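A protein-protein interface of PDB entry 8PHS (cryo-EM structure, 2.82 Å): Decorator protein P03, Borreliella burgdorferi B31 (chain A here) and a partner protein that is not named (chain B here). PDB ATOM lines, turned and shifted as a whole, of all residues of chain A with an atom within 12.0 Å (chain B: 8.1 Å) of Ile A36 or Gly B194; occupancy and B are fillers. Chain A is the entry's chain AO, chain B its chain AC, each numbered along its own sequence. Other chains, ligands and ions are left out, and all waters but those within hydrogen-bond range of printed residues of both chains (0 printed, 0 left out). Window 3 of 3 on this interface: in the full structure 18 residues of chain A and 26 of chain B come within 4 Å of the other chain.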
ATOM      1  N   LEU A  32       0.604 -10.185  -0.733  1.00  0.00           N
ATOM      2  CA  LEU A  32       0.602 -11.448  -0.012  1.00  0.00           C
ATOM      3  C   LEU A  32       1.177 -12.540  -0.904  1.00  0.00           C
ATOM      4  O   LEU A  32       0.873 -12.602  -2.099  1.00  0.00           O
ATOM      5  CB  LEU A  32      -0.813 -11.826   0.429  1.00  0.00           C
ATOM      6  CG  LEU A  32      -1.555 -10.844   1.335  1.00  0.00           C
ATOM      7  CD1 LEU A  32      -3.004 -11.266   1.501  1.00  0.00           C
ATOM      8  CD2 LEU A  32      -0.875 -10.752   2.687  1.00  0.00           C
ATOM      9  N   SER A  33       2.015 -13.393  -0.322  1.00  0.00           N
ATOM     10  CA  SER A  33       2.603 -14.489  -1.078  1.00  0.00           C
ATOM     11  C   SER A  33       1.525 -15.474  -1.518  1.00  0.00           C
ATOM     12  O   SER A  33       0.515 -15.672  -0.837  1.00  0.00           O
ATOM     13  CB  SER A  33       3.662 -15.208  -0.242  1.00  0.00           C
ATOM     14  OG  SER A  33       3.079 -15.860   0.872  1.00  0.00           O
ATOM     15  N   ASN A  34       1.747 -16.089  -2.681  1.00  0.00           N
ATOM     16  CA  ASN A  34       0.776 -17.044  -3.204  1.00  0.00           C
ATOM     17  C   ASN A  34       0.883 -18.394  -2.505  1.00  0.00           C
ATOM     18  O   ASN A  34      -0.141 -19.013  -2.191  1.00  0.00           O
ATOM     19  CB  ASN A  34       0.961 -17.209  -4.712  1.00  0.00           C
ATOM     20  CG  ASN A  34      -0.341 -17.499  -5.428  1.00  0.00           C
ATOM     21  OD1 ASN A  34      -1.405 -17.551  -4.811  1.00  0.00           O
ATOM     22  ND2 ASN A  34      -0.265 -17.693  -6.739  1.00  0.00           N
ATOM     23  N   SER A  35       2.109 -18.855  -2.247  1.00  0.00           N
ATOM     24  CA  SER A  35       2.368 -20.121  -1.560  1.00  0.00           C
ATOM     25  C   SER A  35       1.603 -21.277  -2.204  1.00  0.00           C
ATOM     26  O   SER A  35       0.966 -22.089  -1.531  1.00  0.00           O
ATOM     27  CB  SER A  35       2.043 -20.014  -0.068  1.00  0.00           C
ATOM     28  OG  SER A  35       0.688 -19.666   0.149  1.00  0.00           O
ATOM     29  N   ILE A  36       1.668 -21.343  -3.533  1.00  0.00           N
ATOM     30  CA  ILE A  36       1.007 -22.401  -4.275  1.00  0.00           C
ATOM     31  C   ILE A  36       1.996 -23.359  -4.934  1.00  0.00           C
ATOM     32  O   ILE A  36       1.655 -24.527  -5.150  1.00  0.00           O
ATOM     33  CB  ILE A  36       0.034 -21.813  -5.322  1.00  0.00           C
ATOM     34  CG1 ILE A  36      -0.937 -22.888  -5.816  1.00  0.00           C
ATOM     35  CG2 ILE A  36       0.795 -21.194  -6.486  1.00  0.00           C
ATOM     36  CD1 ILE A  36      -1.842 -23.429  -4.734  1.00  0.00           C
ATOM     37  N   ASP A  37       3.207 -22.911  -5.243  1.00  0.00           N
ATOM     38  CA  ASP A  37       4.223 -23.757  -5.848  1.00  0.00           C
ATOM     39  C   ASP A  37       5.287 -24.118  -4.815  1.00  0.00           C
ATOM     40  O   ASP A  37       5.383 -23.516  -3.744  1.00  0.00           O
ATOM     41  CB  ASP A  37       4.855 -23.057  -7.055  1.00  0.00           C
ATOM     42  CG  ASP A  37       5.500 -24.029  -8.021  1.00  0.00           C
ATOM     43  OD1 ASP A  37       5.381 -25.253  -7.803  1.00  0.00           O
ATOM     44  OD2 ASP A  37       6.128 -23.571  -8.998  1.00  0.00           O
ATOM     45  N   PHE A  38       6.094 -25.123  -5.154  1.00  0.00           N
ATOM     46  CA  PHE A  38       7.150 -25.591  -4.270  1.00  0.00           C
ATOM     47  C   PHE A  38       8.529 -25.564  -4.912  1.00  0.00           C
ATOM     48  O   PHE A  38       9.504 -25.937  -4.251  1.00  0.00           O
ATOM     49  CB  PHE A  38       6.858 -27.019  -3.781  1.00  0.00           C
ATOM     50  CG  PHE A  38       6.888 -28.054  -4.871  1.00  0.00           C
ATOM     51  CD1 PHE A  38       5.850 -28.156  -5.784  1.00  0.00           C
ATOM     52  CD2 PHE A  38       7.964 -28.917  -4.990  1.00  0.00           C
ATOM     53  CE1 PHE A  38       5.883 -29.104  -6.786  1.00  0.00           C
ATOM     54  CE2 PHE A  38       8.001 -29.865  -5.992  1.00  0.00           C
ATOM     55  CZ  PHE A  38       6.961 -29.959  -6.890  1.00  0.00           C
ATOM     56  N   ARG A  39       8.641 -25.139  -6.165  1.00  0.00           N
ATOM     57  CA  ARG A  39       9.906 -25.158  -6.886  1.00  0.00           C
ATOM     58  C   ARG A  39      10.517 -23.764  -6.929  1.00  0.00           C
ATOM     59  O   ARG A  39       9.812 -22.772  -7.142  1.00  0.00           O
ATOM     60  CB  ARG A  39       9.713 -25.687  -8.308  1.00  0.00           C
ATOM     61  CG  ARG A  39       9.130 -27.088  -8.374  1.00  0.00           C
ATOM     62  CD  ARG A  39       8.641 -27.414  -9.774  1.00  0.00           C
ATOM     63  NE  ARG A  39       7.656 -26.447 -10.243  1.00  0.00           N
ATOM     64  CZ  ARG A  39       6.409 -26.749 -10.576  1.00  0.00           C
ATOM     65  NH1 ARG A  39       5.956 -27.990 -10.510  1.00  0.00           N
ATOM     66  NH2 ARG A  39       5.595 -25.780 -10.987  1.00  0.00           N
ATOM     67  N   ASP A  40      11.832 -23.701  -6.726  1.00  0.00           N
ATOM     68  CA  ASP A  40      12.602 -22.459  -6.786  1.00  0.00           C
ATOM     69  C   ASP A  40      12.040 -21.410  -5.825  1.00  0.00           C
ATOM     70  O   ASP A  40      11.665 -20.302  -6.211  1.00  0.00           O
ATOM     71  CB  ASP A  40      12.662 -21.923  -8.219  1.00  0.00           C
ATOM     72  CG  ASP A  40      13.473 -22.814  -9.137  1.00  0.00           C
ATOM     73  OD1 ASP A  40      14.048 -23.806  -8.643  1.00  0.00           O
ATOM     74  OD2 ASP A  40      13.537 -22.524 -10.350  1.00  0.00           O
ATOM     75  N   GLN A  41      11.987 -21.786  -4.548  1.00  0.00           N
ATOM     76  CA  GLN A  41      11.533 -20.892  -3.490  1.00  0.00           C
ATOM     77  C   GLN A  41      12.609 -20.640  -2.440  1.00  0.00           C
ATOM     78  O   GLN A  41      12.339 -19.956  -1.445  1.00  0.00           O
ATOM     79  CB  GLN A  41      10.273 -21.450  -2.823  1.00  0.00           C
ATOM     80  CG  GLN A  41       9.184 -21.872  -3.794  1.00  0.00           C
ATOM     81  CD  GLN A  41       8.473 -20.691  -4.421  1.00  0.00           C
ATOM     82  OE1 GLN A  41       7.865 -19.877  -3.726  1.00  0.00           O
ATOM     83  NE2 GLN A  41       8.543 -20.592  -5.743  1.00  0.00           N
ATOM     84  N   LYS B  48       3.092 -12.823   7.508  1.00  0.00           N
ATOM     85  CA  LYS B  48       2.812 -14.103   6.874  1.00  0.00           C
ATOM     86  C   LYS B  48       4.076 -14.947   6.867  1.00  0.00           C
ATOM     87  O   LYS B  48       5.181 -14.424   6.707  1.00  0.00           O
ATOM     88  CB  LYS B  48       2.284 -13.922   5.446  1.00  0.00           C
ATOM     89  CG  LYS B  48       1.834 -15.216   4.786  1.00  0.00           C
ATOM     90  CD  LYS B  48       1.034 -14.951   3.525  1.00  0.00           C
ATOM     91  CE  LYS B  48       0.491 -16.244   2.938  1.00  0.00           C
ATOM     92  NZ  LYS B  48      -0.400 -15.996   1.772  1.00  0.00           N
ATOM     93  N   ASP B  50       6.150 -18.464   5.396  1.00  0.00           N
ATOM     94  CA  ASP B  50       6.254 -19.346   4.243  1.00  0.00           C
ATOM     95  C   ASP B  50       7.399 -20.323   4.464  1.00  0.00           C
ATOM     96  O   ASP B  50       8.342 -20.045   5.207  1.00  0.00           O
ATOM     97  CB  ASP B  50       6.471 -18.555   2.948  1.00  0.00           C
ATOM     98  CG  ASP B  50       6.128 -19.357   1.710  1.00  0.00           C
ATOM     99  OD1 ASP B  50       5.863 -20.570   1.839  1.00  0.00           O
ATOM    100  OD2 ASP B  50       6.121 -18.774   0.605  1.00  0.00           O
ATOM    101  N   LEU B 191      -2.948 -17.268 -14.703  1.00  0.00           N
ATOM    102  CA  LEU B 191      -3.530 -16.976 -13.398  1.00  0.00           C
ATOM    103  C   LEU B 191      -3.341 -18.148 -12.441  1.00  0.00           C
ATOM    104  O   LEU B 191      -3.300 -19.312 -12.845  1.00  0.00           O
ATOM    105  CB  LEU B 191      -5.020 -16.658 -13.529  1.00  0.00           C
ATOM    106  CG  LEU B 191      -5.442 -15.192 -13.617  1.00  0.00           C
ATOM    107  CD1 LEU B 191      -6.919 -15.087 -13.938  1.00  0.00           C
ATOM    108  CD2 LEU B 191      -5.140 -14.482 -12.314  1.00  0.00           C
ATOM    109  N   GLU B 192      -3.222 -17.827 -11.150  1.00  0.00           N
ATOM    110  CA  GLU B 192      -3.036 -18.829 -10.093  1.00  0.00           C
ATOM    111  C   GLU B 192      -3.983 -18.484  -8.944  1.00  0.00           C
ATOM    112  O   GLU B 192      -3.653 -17.669  -8.079  1.00  0.00           O
ATOM    113  CB  GLU B 192      -1.588 -18.883  -9.626  1.00  0.00           C
ATOM    114  CG  GLU B 192      -0.586 -19.203 -10.720  1.00  0.00           C
ATOM    115  CD  GLU B 192       0.843 -18.967 -10.282  1.00  0.00           C
ATOM    116  OE1 GLU B 192       1.049 -18.549  -9.122  1.00  0.00           O
ATOM    117  OE2 GLU B 192       1.762 -19.201 -11.094  1.00  0.00           O
ATOM    118  N   LEU B 193      -5.157 -19.114  -8.938  1.00  0.00           N
ATOM    119  CA  LEU B 193      -6.140 -18.897  -7.885  1.00  0.00           C
ATOM    120  C   LEU B 193      -5.983 -19.851  -6.709  1.00  0.00           C
ATOM    121  O   LEU B 193      -6.660 -19.668  -5.691  1.00  0.00           O
ATOM    122  CB  LEU B 193      -7.557 -19.021  -8.450  1.00  0.00           C
ATOM    123  CG  LEU B 193      -7.934 -18.021  -9.543  1.00  0.00           C
ATOM    124  CD1 LEU B 193      -9.417 -18.108  -9.852  1.00  0.00           C
ATOM    125  CD2 LEU B 193      -7.552 -16.609  -9.128  1.00  0.00           C
ATOM    126  N   GLY B 194      -5.116 -20.857  -6.820  1.00  0.00           N
ATOM    127  CA  GLY B 194      -4.900 -21.775  -5.719  1.00  0.00           C
ATOM    128  C   GLY B 194      -6.132 -22.603  -5.394  1.00  0.00           C
ATOM    129  O   GLY B 194      -6.922 -22.972  -6.269  1.00  0.00           O
ATOM    130  N   ASP B 195      -6.293 -22.902  -4.105  1.00  0.00           N
ATOM    131  CA  ASP B 195      -7.433 -23.682  -3.637  1.00  0.00           C
ATOM    132  C   ASP B 195      -8.698 -22.850  -3.487  1.00  0.00           C
ATOM    133  O   ASP B 195      -9.773 -23.420  -3.265  1.00  0.00           O
ATOM    134  CB  ASP B 195      -7.098 -24.353  -2.302  1.00  0.00           C
ATOM    135  CG  ASP B 195      -6.017 -25.408  -2.438  1.00  0.00           C
ATOM    136  OD1 ASP B 195      -5.506 -25.595  -3.561  1.00  0.00           O
ATOM    137  OD2 ASP B 195      -5.679 -26.048  -1.420  1.00  0.00           O
ATOM    138  N   GLU B 196      -8.601 -21.523  -3.601  1.00  0.00           N
ATOM    139  CA  GLU B 196      -9.761 -20.640  -3.570  1.00  0.00           C
ATOM    140  C   GLU B 196     -10.326 -20.377  -4.959  1.00  0.00           C
ATOM    141  O   GLU B 196     -10.928 -19.320  -5.191  1.00  0.00           O
ATOM    142  CB  GLU B 196      -9.396 -19.322  -2.885  1.00  0.00           C
ATOM    143  CG  GLU B 196      -9.104 -19.447  -1.397  1.00  0.00           C
ATOM    144  CD  GLU B 196     -10.363 -19.509  -0.555  1.00  0.00           C
ATOM    145  OE1 GLU B 196     -11.470 -19.372  -1.120  1.00  0.00           O
ATOM    146  OE2 GLU B 196     -10.247 -19.692   0.675  1.00  0.00           O
ATOM    147  N   PHE B 197     -10.141 -21.315  -5.891  1.00  0.00           N
ATOM    148  CA  PHE B 197     -10.579 -21.108  -7.268  1.00  0.00           C
ATOM    149  C   PHE B 197     -12.097 -21.030  -7.384  1.00  0.00           C
ATOM    150  O   PHE B 197     -12.611 -20.284  -8.225  1.00  0.00           O
ATOM    151  CB  PHE B 197     -10.034 -22.221  -8.165  1.00  0.00           C
ATOM    152  CG  PHE B 197     -10.634 -23.574  -7.894  1.00  0.00           C
ATOM    153  CD1 PHE B 197     -10.283 -24.290  -6.760  1.00  0.00           C
ATOM    154  CD2 PHE B 197     -11.547 -24.130  -8.772  1.00  0.00           C
ATOM    155  CE1 PHE B 197     -10.833 -25.533  -6.509  1.00  0.00           C
ATOM    156  CE2 PHE B 197     -12.100 -25.373  -8.526  1.00  0.00           C
ATOM    157  CZ  PHE B 197     -11.741 -26.074  -7.393  1.00  0.00           C
ATOM    158  N   SER B 198     -12.828 -21.778  -6.560  1.00  0.00           N
ATOM    159  CA  SER B 198     -14.290 -21.799  -6.626  1.00  0.00           C
ATOM    160  C   SER B 198     -14.828 -20.496  -6.041  1.00  0.00           C
ATOM    161  O   SER B 198     -15.231 -20.411  -4.879  1.00  0.00           O
ATOM    162  CB  SER B 198     -14.845 -23.012  -5.891  1.00  0.00           C
ATOM    163  OG  SER B 198     -16.261 -22.985  -5.864  1.00  0.00           O
ATOM    164  N   ILE B 241     -12.078 -21.789 -15.453  1.00  0.00           N
ATOM    165  CA  ILE B 241     -11.087 -21.654 -14.389  1.00  0.00           C
ATOM    166  C   ILE B 241     -11.705 -21.356 -13.027  1.00  0.00           C
ATOM    167  O   ILE B 241     -11.068 -21.641 -12.002  1.00  0.00           O
ATOM    168  CB  ILE B 241     -10.035 -20.578 -14.729  1.00  0.00           C
ATOM    169  CG1 ILE B 241     -10.564 -19.178 -14.415  1.00  0.00           C
ATOM    170  CG2 ILE B 241      -9.617 -20.679 -16.181  1.00  0.00           C
ATOM    171  CD1 ILE B 241      -9.504 -18.106 -14.460  1.00  0.00           C
ATOM    172  N   LEU B 268      -8.400 -13.679  -1.253  1.00  0.00           N
ATOM    173  CA  LEU B 268      -7.375 -13.288  -2.212  1.00  0.00           C
ATOM    174  C   LEU B 268      -7.205 -11.777  -2.306  1.00  0.00           C
ATOM    175  O   LEU B 268      -6.079 -11.275  -2.242  1.00  0.00           O
ATOM    176  CB  LEU B 268      -7.706 -13.864  -3.592  1.00  0.00           C
ATOM    177  CG  LEU B 268      -7.690 -15.390  -3.699  1.00  0.00           C
ATOM    178  CD1 LEU B 268      -8.118 -15.836  -5.084  1.00  0.00           C
ATOM    179  CD2 LEU B 268      -6.312 -15.935  -3.360  1.00  0.00           C
ATOM    180  N   ARG B 308      -0.508 -12.303  -4.733  1.00  0.00           N
ATOM    181  CA  ARG B 308       0.263 -12.243  -5.965  1.00  0.00           C
ATOM    182  C   ARG B 308      -0.345 -13.138  -7.038  1.00  0.00           C
ATOM    183  O   ARG B 308      -0.876 -14.216  -6.757  1.00  0.00           O
ATOM    184  CB  ARG B 308       1.714 -12.650  -5.710  1.00  0.00           C
ATOM    185  CG  ARG B 308       2.492 -11.652  -4.873  1.00  0.00           C
ATOM    186  CD  ARG B 308       3.983 -11.919  -4.943  1.00  0.00           C
ATOM    187  NE  ARG B 308       4.751 -10.877  -4.273  1.00  0.00           N
ATOM    188  CZ  ARG B 308       6.076 -10.806  -4.272  1.00  0.00           C
ATOM    189  NH1 ARG B 308       6.816 -11.700  -4.907  1.00  0.00           N
ATOM    190  NH2 ARG B 308       6.671  -9.812  -3.619  1.00  0.00           N
ATOM    191  N   LYS B 309      -0.259 -12.669  -8.284  1.00  0.00           N
ATOM    192  CA  LYS B 309      -0.699 -13.422  -9.461  1.00  0.00           C
ATOM    193  C   LYS B 309      -2.167 -13.834  -9.355  1.00  0.00           C
ATOM    194  O   LYS B 309      -2.534 -14.983  -9.606  1.00  0.00           O
ATOM    195  CB  LYS B 309       0.198 -14.638  -9.699  1.00  0.00           C
ATOM    196  CG  LYS B 309       1.601 -14.286 -10.156  1.00  0.00           C
ATOM    197  CD  LYS B 309       2.439 -15.535 -10.374  1.00  0.00           C
ATOM    198  CE  LYS B 309       3.820 -15.184 -10.905  1.00  0.00           C
ATOM    199  NZ  LYS B 309       4.681 -16.389 -11.061  1.00  0.00           N
ATOM    200  N   THR B 310      -3.017 -12.877  -8.979  1.00  0.00           N
ATOM    201  CA  THR B 310      -4.456 -13.102  -8.947  1.00  0.00           C
ATOM    202  C   THR B 310      -5.229 -12.040  -9.720  1.00  0.00           C
ATOM    203  O   THR B 310      -6.462 -12.017  -9.649  1.00  0.00           O
ATOM    204  CB  THR B 310      -4.970 -13.165  -7.506  1.00  0.00           C
ATOM    205  OG1 THR B 310      -4.488 -12.034  -6.772  1.00  0.00           O
ATOM    206  CG2 THR B 310      -4.500 -14.443  -6.832  1.00  0.00           C
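Of the 10 printed residues of chain A, 4 touch a printed residue of chain B. Hydrophobic or aromatic side chains of chain A within 4 Å of the printed part of chain B: Ile A36. Along chain A the printed residues that touch a printed residue of chain B span positions 32 to 36. Among the printed residues, no Asp or Glu carboxylate lies within 4 Å of a Lys or Arg side-chain nitrogen of the other chain.
Arg B308 touches Asn A34. CG2 of Ile A36 touches OE1 of Glu B192 (3.7 Å). CD1 of Ile A36 touches CA of Gly B194, at 3.6 Å.
Of the printed residues of chain B, Asn A34 touches Glu B192 (2.9 Å) and Arg B308 (3.5 Å). Ile A36 touches just these residues of chain B: Glu B192 (3.7 Å) and Gly B194 (3.6 Å). Of chain A, only Asn A34 and Ile A36 come within 4 Å of Glu B192. Leu B193 touches none of the printed residues of chain A. Gly B194 touches just one residue of chain A: Ile A36. No residue of chain A comes within 4 Å of Asp B195. No residue of chain A comes within 4 Å of Glu B196. Printed residues of chain A within 4 Å of Arg B308: Leu A32 and Asn A34. The nearest residue of chain A that does not touch Gly B194 is Asn A34 (5.4 Å). The nearest printed residue of chain B that does not touch Leu A32 is Lys B48 (4.4 Å).
The side-chain amino group (NZ) of Lys B48 is in hydrogen-bond range of the backbone carbonyl oxygen (O) of Ser A33, 2.8 Å away. OE1 of Glu B192 is in hydrogen-bond range of ND2 of Asn A34 (2.9 Å). The backbone carbonyl oxygen (O) of Leu A32 lies within hydrogen-bond range of the backbone NH (N) of Arg B308 (3.0 Å).
The backbone carbonyl oxygen (O) of Lys B309 is in hydrogen-bond range of the backbone NH (N) of Glu B192 (3.3 Å).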
